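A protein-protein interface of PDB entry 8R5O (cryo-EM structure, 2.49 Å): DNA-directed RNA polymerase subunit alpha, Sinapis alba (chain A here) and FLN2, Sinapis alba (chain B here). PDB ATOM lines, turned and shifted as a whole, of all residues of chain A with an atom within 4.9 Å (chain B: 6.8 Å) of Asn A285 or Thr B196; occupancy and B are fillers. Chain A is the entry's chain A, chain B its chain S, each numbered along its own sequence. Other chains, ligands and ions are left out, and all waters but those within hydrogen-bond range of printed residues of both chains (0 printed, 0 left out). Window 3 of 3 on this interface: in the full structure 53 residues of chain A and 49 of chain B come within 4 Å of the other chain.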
ATOM      1  N   PRO A 281     -13.129   0.716   3.691  1.00  0.00           N
ATOM      2  CA  PRO A 281     -12.681   2.059   4.095  1.00  0.00           C
ATOM      3  C   PRO A 281     -12.071   2.114   5.484  1.00  0.00           C
ATOM      4  O   PRO A 281     -11.155   2.913   5.712  1.00  0.00           O
ATOM      5  CB  PRO A 281     -13.966   2.896   4.008  1.00  0.00           C
ATOM      6  CG  PRO A 281     -15.076   1.904   4.104  1.00  0.00           C
ATOM      7  CD  PRO A 281     -14.575   0.674   3.416  1.00  0.00           C
ATOM      8  N   ARG A 282     -12.550   1.298   6.425  1.00  0.00           N
ATOM      9  CA  ARG A 282     -11.958   1.294   7.758  1.00  0.00           C
ATOM     10  C   ARG A 282     -10.528   0.767   7.725  1.00  0.00           C
ATOM     11  O   ARG A 282      -9.650   1.293   8.419  1.00  0.00           O
ATOM     12  CB  ARG A 282     -12.819   0.469   8.713  1.00  0.00           C
ATOM     13  CG  ARG A 282     -12.382   0.553  10.165  1.00  0.00           C
ATOM     14  CD  ARG A 282     -13.242  -0.333  11.046  1.00  0.00           C
ATOM     15  NE  ARG A 282     -13.437  -1.649  10.451  1.00  0.00           N
ATOM     16  CZ  ARG A 282     -12.595  -2.665  10.584  1.00  0.00           C
ATOM     17  NH1 ARG A 282     -11.487  -2.555  11.297  1.00  0.00           N
ATOM     18  NH2 ARG A 282     -12.873  -3.820   9.986  1.00  0.00           N
ATOM     19  N   ILE A 283     -10.276  -0.273   6.926  1.00  0.00           N
ATOM     20  CA  ILE A 283      -8.915  -0.783   6.768  1.00  0.00           C
ATOM     21  C   ILE A 283      -8.033   0.256   6.091  1.00  0.00           C
ATOM     22  O   ILE A 283      -6.880   0.469   6.485  1.00  0.00           O
ATOM     23  CB  ILE A 283      -8.926  -2.114   5.988  1.00  0.00           C
ATOM     24  CG1 ILE A 283      -9.383  -3.269   6.882  1.00  0.00           C
ATOM     25  CG2 ILE A 283      -7.551  -2.414   5.404  1.00  0.00           C
ATOM     26  CD1 ILE A 283     -10.881  -3.396   7.029  1.00  0.00           C
ATOM     27  N   TYR A 284      -8.563   0.925   5.062  1.00  0.00           N
ATOM     28  CA  TYR A 284      -7.778   1.911   4.326  1.00  0.00           C
ATOM     29  C   TYR A 284      -7.327   3.051   5.228  1.00  0.00           C
ATOM     30  O   TYR A 284      -6.178   3.500   5.143  1.00  0.00           O
ATOM     31  CB  TYR A 284      -8.594   2.449   3.148  1.00  0.00           C
ATOM     32  CG  TYR A 284      -7.917   3.562   2.375  1.00  0.00           C
ATOM     33  CD1 TYR A 284      -7.043   3.278   1.335  1.00  0.00           C
ATOM     34  CD2 TYR A 284      -8.166   4.895   2.673  1.00  0.00           C
ATOM     35  CE1 TYR A 284      -6.426   4.290   0.626  1.00  0.00           C
ATOM     36  CE2 TYR A 284      -7.554   5.911   1.971  1.00  0.00           C
ATOM     37  CZ  TYR A 284      -6.687   5.605   0.949  1.00  0.00           C
ATOM     38  OH  TYR A 284      -6.079   6.617   0.249  1.00  0.00           O
ATOM     39  N   ASN A 285      -8.218   3.540   6.092  1.00  0.00           N
ATOM     40  CA  ASN A 285      -7.856   4.643   6.975  1.00  0.00           C
ATOM     41  C   ASN A 285      -6.766   4.243   7.960  1.00  0.00           C
ATOM     42  O   ASN A 285      -5.898   5.058   8.285  1.00  0.00           O
ATOM     43  CB  ASN A 285      -9.090   5.152   7.722  1.00  0.00           C
ATOM     44  CG  ASN A 285     -10.080   5.844   6.806  1.00  0.00           C
ATOM     45  OD1 ASN A 285      -9.741   6.238   5.691  1.00  0.00           O
ATOM     46  ND2 ASN A 285     -11.310   6.003   7.278  1.00  0.00           N
ATOM     47  N   CYS A 286      -6.791   3.001   8.445  1.00  0.00           N
ATOM     48  CA  CYS A 286      -5.751   2.540   9.361  1.00  0.00           C
ATOM     49  C   CYS A 286      -4.387   2.506   8.683  1.00  0.00           C
ATOM     50  O   CYS A 286      -3.384   2.939   9.261  1.00  0.00           O
ATOM     51  CB  CYS A 286      -6.111   1.163   9.917  1.00  0.00           C
ATOM     52  SG  CYS A 286      -7.590   1.137  10.953  1.00  0.00           S
ATOM     53  N   LEU A 287      -4.326   1.986   7.453  1.00  0.00           N
ATOM     54  CA  LEU A 287      -3.049   1.899   6.751  1.00  0.00           C
ATOM     55  C   LEU A 287      -2.500   3.282   6.416  1.00  0.00           C
ATOM     56  O   LEU A 287      -1.291   3.520   6.532  1.00  0.00           O
ATOM     57  CB  LEU A 287      -3.202   1.056   5.484  1.00  0.00           C
ATOM     58  CG  LEU A 287      -3.651  -0.396   5.667  1.00  0.00           C
ATOM     59  CD1 LEU A 287      -3.644  -1.142   4.344  1.00  0.00           C
ATOM     60  CD2 LEU A 287      -2.780  -1.106   6.691  1.00  0.00           C
ATOM     61  N   LYS A 288      -3.368   4.207   5.998  1.00  0.00           N
ATOM     62  CA  LYS A 288      -2.919   5.567   5.715  1.00  0.00           C
ATOM     63  C   LYS A 288      -2.499   6.285   6.990  1.00  0.00           C
ATOM     64  O   LYS A 288      -1.549   7.076   6.981  1.00  0.00           O
ATOM     65  CB  LYS A 288      -4.020   6.346   4.994  1.00  0.00           C
ATOM     66  CG  LYS A 288      -4.014   6.200   3.475  1.00  0.00           C
ATOM     67  CD  LYS A 288      -2.905   7.028   2.844  1.00  0.00           C
ATOM     68  CE  LYS A 288      -3.058   7.121   1.334  1.00  0.00           C
ATOM     69  NZ  LYS A 288      -2.919   5.800   0.663  1.00  0.00           N
ATOM     70  N   LYS A 289      -3.203   6.027   8.096  1.00  0.00           N
ATOM     71  CA  LYS A 289      -2.844   6.634   9.374  1.00  0.00           C
ATOM     72  C   LYS A 289      -1.455   6.204   9.825  1.00  0.00           C
ATOM     73  O   LYS A 289      -0.756   6.966  10.499  1.00  0.00           O
ATOM     74  CB  LYS A 289      -3.890   6.273  10.429  1.00  0.00           C
ATOM     75  CG  LYS A 289      -3.800   7.064  11.724  1.00  0.00           C
ATOM     76  CD  LYS A 289      -4.947   6.695  12.653  1.00  0.00           C
ATOM     77  CE  LYS A 289      -4.937   7.531  13.920  1.00  0.00           C
ATOM     78  NZ  LYS A 289      -6.131   7.254  14.762  1.00  0.00           N
ATOM     79  N   HIS A 311      -7.815  -0.064  16.007  1.00  0.00           N
ATOM     80  CA  HIS A 311      -9.007  -0.366  15.215  1.00  0.00           C
ATOM     81  C   HIS A 311      -8.775  -1.456  14.177  1.00  0.00           C
ATOM     82  O   HIS A 311      -9.719  -1.822  13.467  1.00  0.00           O
ATOM     83  CB  HIS A 311      -9.571   0.874  14.506  1.00  0.00           C
ATOM     84  CG  HIS A 311      -9.870   2.014  15.428  1.00  0.00           C
ATOM     85  ND1 HIS A 311     -10.034   3.307  14.980  1.00  0.00           N
ATOM     86  CD2 HIS A 311     -10.036   2.057  16.771  1.00  0.00           C
ATOM     87  CE1 HIS A 311     -10.287   4.098  16.008  1.00  0.00           C
ATOM     88  NE2 HIS A 311     -10.294   3.364  17.105  1.00  0.00           N
ATOM     89  N   ILE B 193     -18.037   4.514  11.078  1.00  0.00           N
ATOM     90  CA  ILE B 193     -16.592   4.515  11.251  1.00  0.00           C
ATOM     91  C   ILE B 193     -16.085   5.935  11.462  1.00  0.00           C
ATOM     92  O   ILE B 193     -14.911   6.225  11.233  1.00  0.00           O
ATOM     93  CB  ILE B 193     -15.889   3.860  10.052  1.00  0.00           C
ATOM     94  CG1 ILE B 193     -16.226   4.607   8.760  1.00  0.00           C
ATOM     95  CG2 ILE B 193     -16.285   2.399   9.945  1.00  0.00           C
ATOM     96  CD1 ILE B 193     -15.544   4.045   7.530  1.00  0.00           C
ATOM     97  N   SER B 194     -16.982   6.819  11.907  1.00  0.00           N
ATOM     98  CA  SER B 194     -16.603   8.203  12.165  1.00  0.00           C
ATOM     99  C   SER B 194     -15.542   8.315  13.252  1.00  0.00           C
ATOM    100  O   SER B 194     -14.856   9.340  13.329  1.00  0.00           O
ATOM    101  CB  SER B 194     -17.834   9.021  12.550  1.00  0.00           C
ATOM    102  OG  SER B 194     -18.449   8.497  13.715  1.00  0.00           O
ATOM    103  N   HIS B 195     -15.396   7.291  14.092  1.00  0.00           N
ATOM    104  CA  HIS B 195     -14.313   7.257  15.067  1.00  0.00           C
ATOM    105  C   HIS B 195     -12.948   7.087  14.416  1.00  0.00           C
ATOM    106  O   HIS B 195     -11.933   7.343  15.071  1.00  0.00           O
ATOM    107  CB  HIS B 195     -14.555   6.131  16.072  1.00  0.00           C
ATOM    108  CG  HIS B 195     -14.674   4.776  15.445  1.00  0.00           C
ATOM    109  ND1 HIS B 195     -13.629   3.879  15.407  1.00  0.00           N
ATOM    110  CD2 HIS B 195     -15.713   4.169  14.824  1.00  0.00           C
ATOM    111  CE1 HIS B 195     -14.020   2.776  14.796  1.00  0.00           C
ATOM    112  NE2 HIS B 195     -15.280   2.928  14.431  1.00  0.00           N
ATOM    113  N   THR B 196     -12.899   6.662  13.153  1.00  0.00           N
ATOM    114  CA  THR B 196     -11.649   6.548  12.417  1.00  0.00           C
ATOM    115  C   THR B 196     -11.327   7.784  11.589  1.00  0.00           C
ATOM    116  O   THR B 196     -10.230   7.863  11.028  1.00  0.00           O
ATOM    117  CB  THR B 196     -11.685   5.324  11.491  1.00  0.00           C
ATOM    118  OG1 THR B 196     -12.802   5.427  10.602  1.00  0.00           O
ATOM    119  CG2 THR B 196     -11.800   4.044  12.301  1.00  0.00           C
ATOM    120  N   TYR B 197     -12.248   8.741  11.494  1.00  0.00           N
ATOM    121  CA  TYR B 197     -11.981   9.960  10.739  1.00  0.00           C
ATOM    122  C   TYR B 197     -10.996  10.833  11.507  1.00  0.00           C
ATOM    123  O   TYR B 197     -11.176  11.088  12.701  1.00  0.00           O
ATOM    124  CB  TYR B 197     -13.275  10.733  10.480  1.00  0.00           C
ATOM    125  CG  TYR B 197     -14.306  10.014   9.637  1.00  0.00           C
ATOM    126  CD1 TYR B 197     -13.987   8.864   8.929  1.00  0.00           C
ATOM    127  CD2 TYR B 197     -15.605  10.496   9.546  1.00  0.00           C
ATOM    128  CE1 TYR B 197     -14.932   8.214   8.163  1.00  0.00           C
ATOM    129  CE2 TYR B 197     -16.556   9.852   8.781  1.00  0.00           C
ATOM    130  CZ  TYR B 197     -16.213   8.712   8.089  1.00  0.00           C
ATOM    131  OH  TYR B 197     -17.155   8.066   7.326  1.00  0.00           O
ATOM    132  N   GLY B 198      -9.958  11.293  10.819  1.00  0.00           N
ATOM    133  CA  GLY B 198      -8.917  12.090  11.424  1.00  0.00           C
ATOM    134  C   GLY B 198      -9.108  13.576  11.202  1.00  0.00           C
ATOM    135  O   GLY B 198     -10.206  14.060  10.907  1.00  0.00           O
ATOM    136  N   LYS B 263      -6.199  17.348   3.445  1.00  0.00           N
ATOM    137  CA  LYS B 263      -6.567  15.972   3.130  1.00  0.00           C
ATOM    138  C   LYS B 263      -7.541  16.017   1.961  1.00  0.00           C
ATOM    139  O   LYS B 263      -8.695  16.427   2.125  1.00  0.00           O
ATOM    140  CB  LYS B 263      -7.183  15.286   4.347  1.00  0.00           C
ATOM    141  CG  LYS B 263      -7.186  13.774   4.298  1.00  0.00           C
ATOM    142  CD  LYS B 263      -7.615  13.206   5.642  1.00  0.00           C
ATOM    143  CE  LYS B 263      -7.440  11.701   5.699  1.00  0.00           C
ATOM    144  NZ  LYS B 263      -7.762  11.166   7.051  1.00  0.00           N
ATOM    145  N   GLN B 289      -5.907  11.087  -2.310  1.00  0.00           N
ATOM    146  CA  GLN B 289      -6.607   9.818  -2.170  1.00  0.00           C
ATOM    147  C   GLN B 289      -7.331   9.484  -3.468  1.00  0.00           C
ATOM    148  O   GLN B 289      -8.146  10.275  -3.952  1.00  0.00           O
ATOM    149  CB  GLN B 289      -7.593   9.876  -1.008  1.00  0.00           C
ATOM    150  CG  GLN B 289      -6.954  10.139   0.336  1.00  0.00           C
ATOM    151  CD  GLN B 289      -7.913   9.916   1.485  1.00  0.00           C
ATOM    152  OE1 GLN B 289      -9.043   9.478   1.288  1.00  0.00           O
ATOM    153  NE2 GLN B 289      -7.464  10.217   2.696  1.00  0.00           N
ATOM    154  N   ARG B 291      -8.917   6.328  -3.932  1.00  0.00           N
ATOM    155  CA  ARG B 291      -9.900   5.267  -3.753  1.00  0.00           C
ATOM    156  C   ARG B 291     -11.240   5.624  -4.381  1.00  0.00           C
ATOM    157  O   ARG B 291     -12.038   4.727  -4.672  1.00  0.00           O
ATOM    158  CB  ARG B 291     -10.074   4.959  -2.265  1.00  0.00           C
ATOM    159  CG  ARG B 291     -10.303   6.188  -1.408  1.00  0.00           C
ATOM    160  CD  ARG B 291     -10.733   5.815  -0.005  1.00  0.00           C
ATOM    161  NE  ARG B 291     -10.850   6.992   0.844  1.00  0.00           N
ATOM    162  CZ  ARG B 291     -11.483   7.021   2.008  1.00  0.00           C
ATOM    163  NH1 ARG B 291     -12.090   5.950   2.490  1.00  0.00           N
ATOM    164  NH2 ARG B 291     -11.511   8.155   2.701  1.00  0.00           N
ATOM    165  N   GLU B 339     -17.232  10.567   4.640  1.00  0.00           N
ATOM    166  CA  GLU B 339     -16.135  11.120   5.427  1.00  0.00           C
ATOM    167  C   GLU B 339     -15.889  12.587   5.092  1.00  0.00           C
ATOM    168  O   GLU B 339     -15.597  13.389   5.987  1.00  0.00           O
ATOM    169  CB  GLU B 339     -14.863  10.302   5.208  1.00  0.00           C
ATOM    170  CG  GLU B 339     -13.661  10.825   5.975  1.00  0.00           C
ATOM    171  CD  GLU B 339     -12.409  10.007   5.739  1.00  0.00           C
ATOM    172  OE1 GLU B 339     -12.486   8.992   5.020  1.00  0.00           O
ATOM    173  OE2 GLU B 339     -11.346  10.383   6.276  1.00  0.00           O
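The backbone carbonyl oxygen (O) of Pro A281 sits close to the side-chain amide nitrogen (ND2) of Asn A285 (3.5 Å).
The guanidinium group (NH1) of Arg A282 sits at hydrogen-bond distance from the backbone carbonyl oxygen (O) of His A311, at 2.9 Å.
The side-chain amino group (NZ) of Lys A288 sits close to the side-chain hydroxyl (OH) of Tyr A284, 3.3 Å away.
NZ of Lys B263 is in salt-bridge range of OE2 of Glu B339 (3.7 Å).
OE1 of Gln B289 lies within hydrogen-bond range of NE of Arg B291 (3.1 Å).
NH2 of Arg B291 is in salt-bridge range of OE1 of Glu B339.
Pro A281 touches Arg B291 (CB to NH1, 3.9 Å).
Tyr A284 touches Gln B289 (OH to CG, 3.6 Å).
Tyr A284 touches Arg B291 (CE2 to NE, 3.6 Å).
OG1 of Thr B196 touches ND2 of Asn A285, 3.7 Å away.
Asn A285 touches Arg B291.
Glu B339 touches Asn A285.
His A311 touches His B195 (CE1 to ND1, 3.4 Å).
Thr B196 touches His A311.
Of chain B, only Thr B196 (3.7 Å), Arg B291 (3.97 Å) and Glu B339 (3.9 Å) come within 4 Å of Asn A285.
Thr B196 touches just these residues of chain A: Asn A285 and His A311.
Printed residues of chain A within 4 Å of Gln B289: Tyr A284.
Of the printed residues of chain B, Tyr A284 touches Gln B289 (3.6 Å) and Arg B291 (3.6 Å).
Printed residues of chain A within 4 Å of Glu B339: Asn A285.
Of the printed residues of chain A, Arg B291 touches Pro A281, Tyr A284 and Asn A285.
Of the printed residues of chain B, Pro A281 touches Arg B291 (3.9 Å).
Lys A289 touches none of the printed residues of chain B.
Cys A286 touches none of the printed residues of chain B.
The nearest residue of chain A that does not touch Thr B196 is Arg A282 (4.1 Å).
The nearest printed residue of chain A that does not touch His B195 is Arg A282 (4.9 Å).
Hydrophobic or aromatic side chains of chain B within 4 Å of the printed part of chain A: His B195.
Printed residues of chain A that touch a printed residue of chain B: Pro A281, Tyr A284, Asn A285 and His A311.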
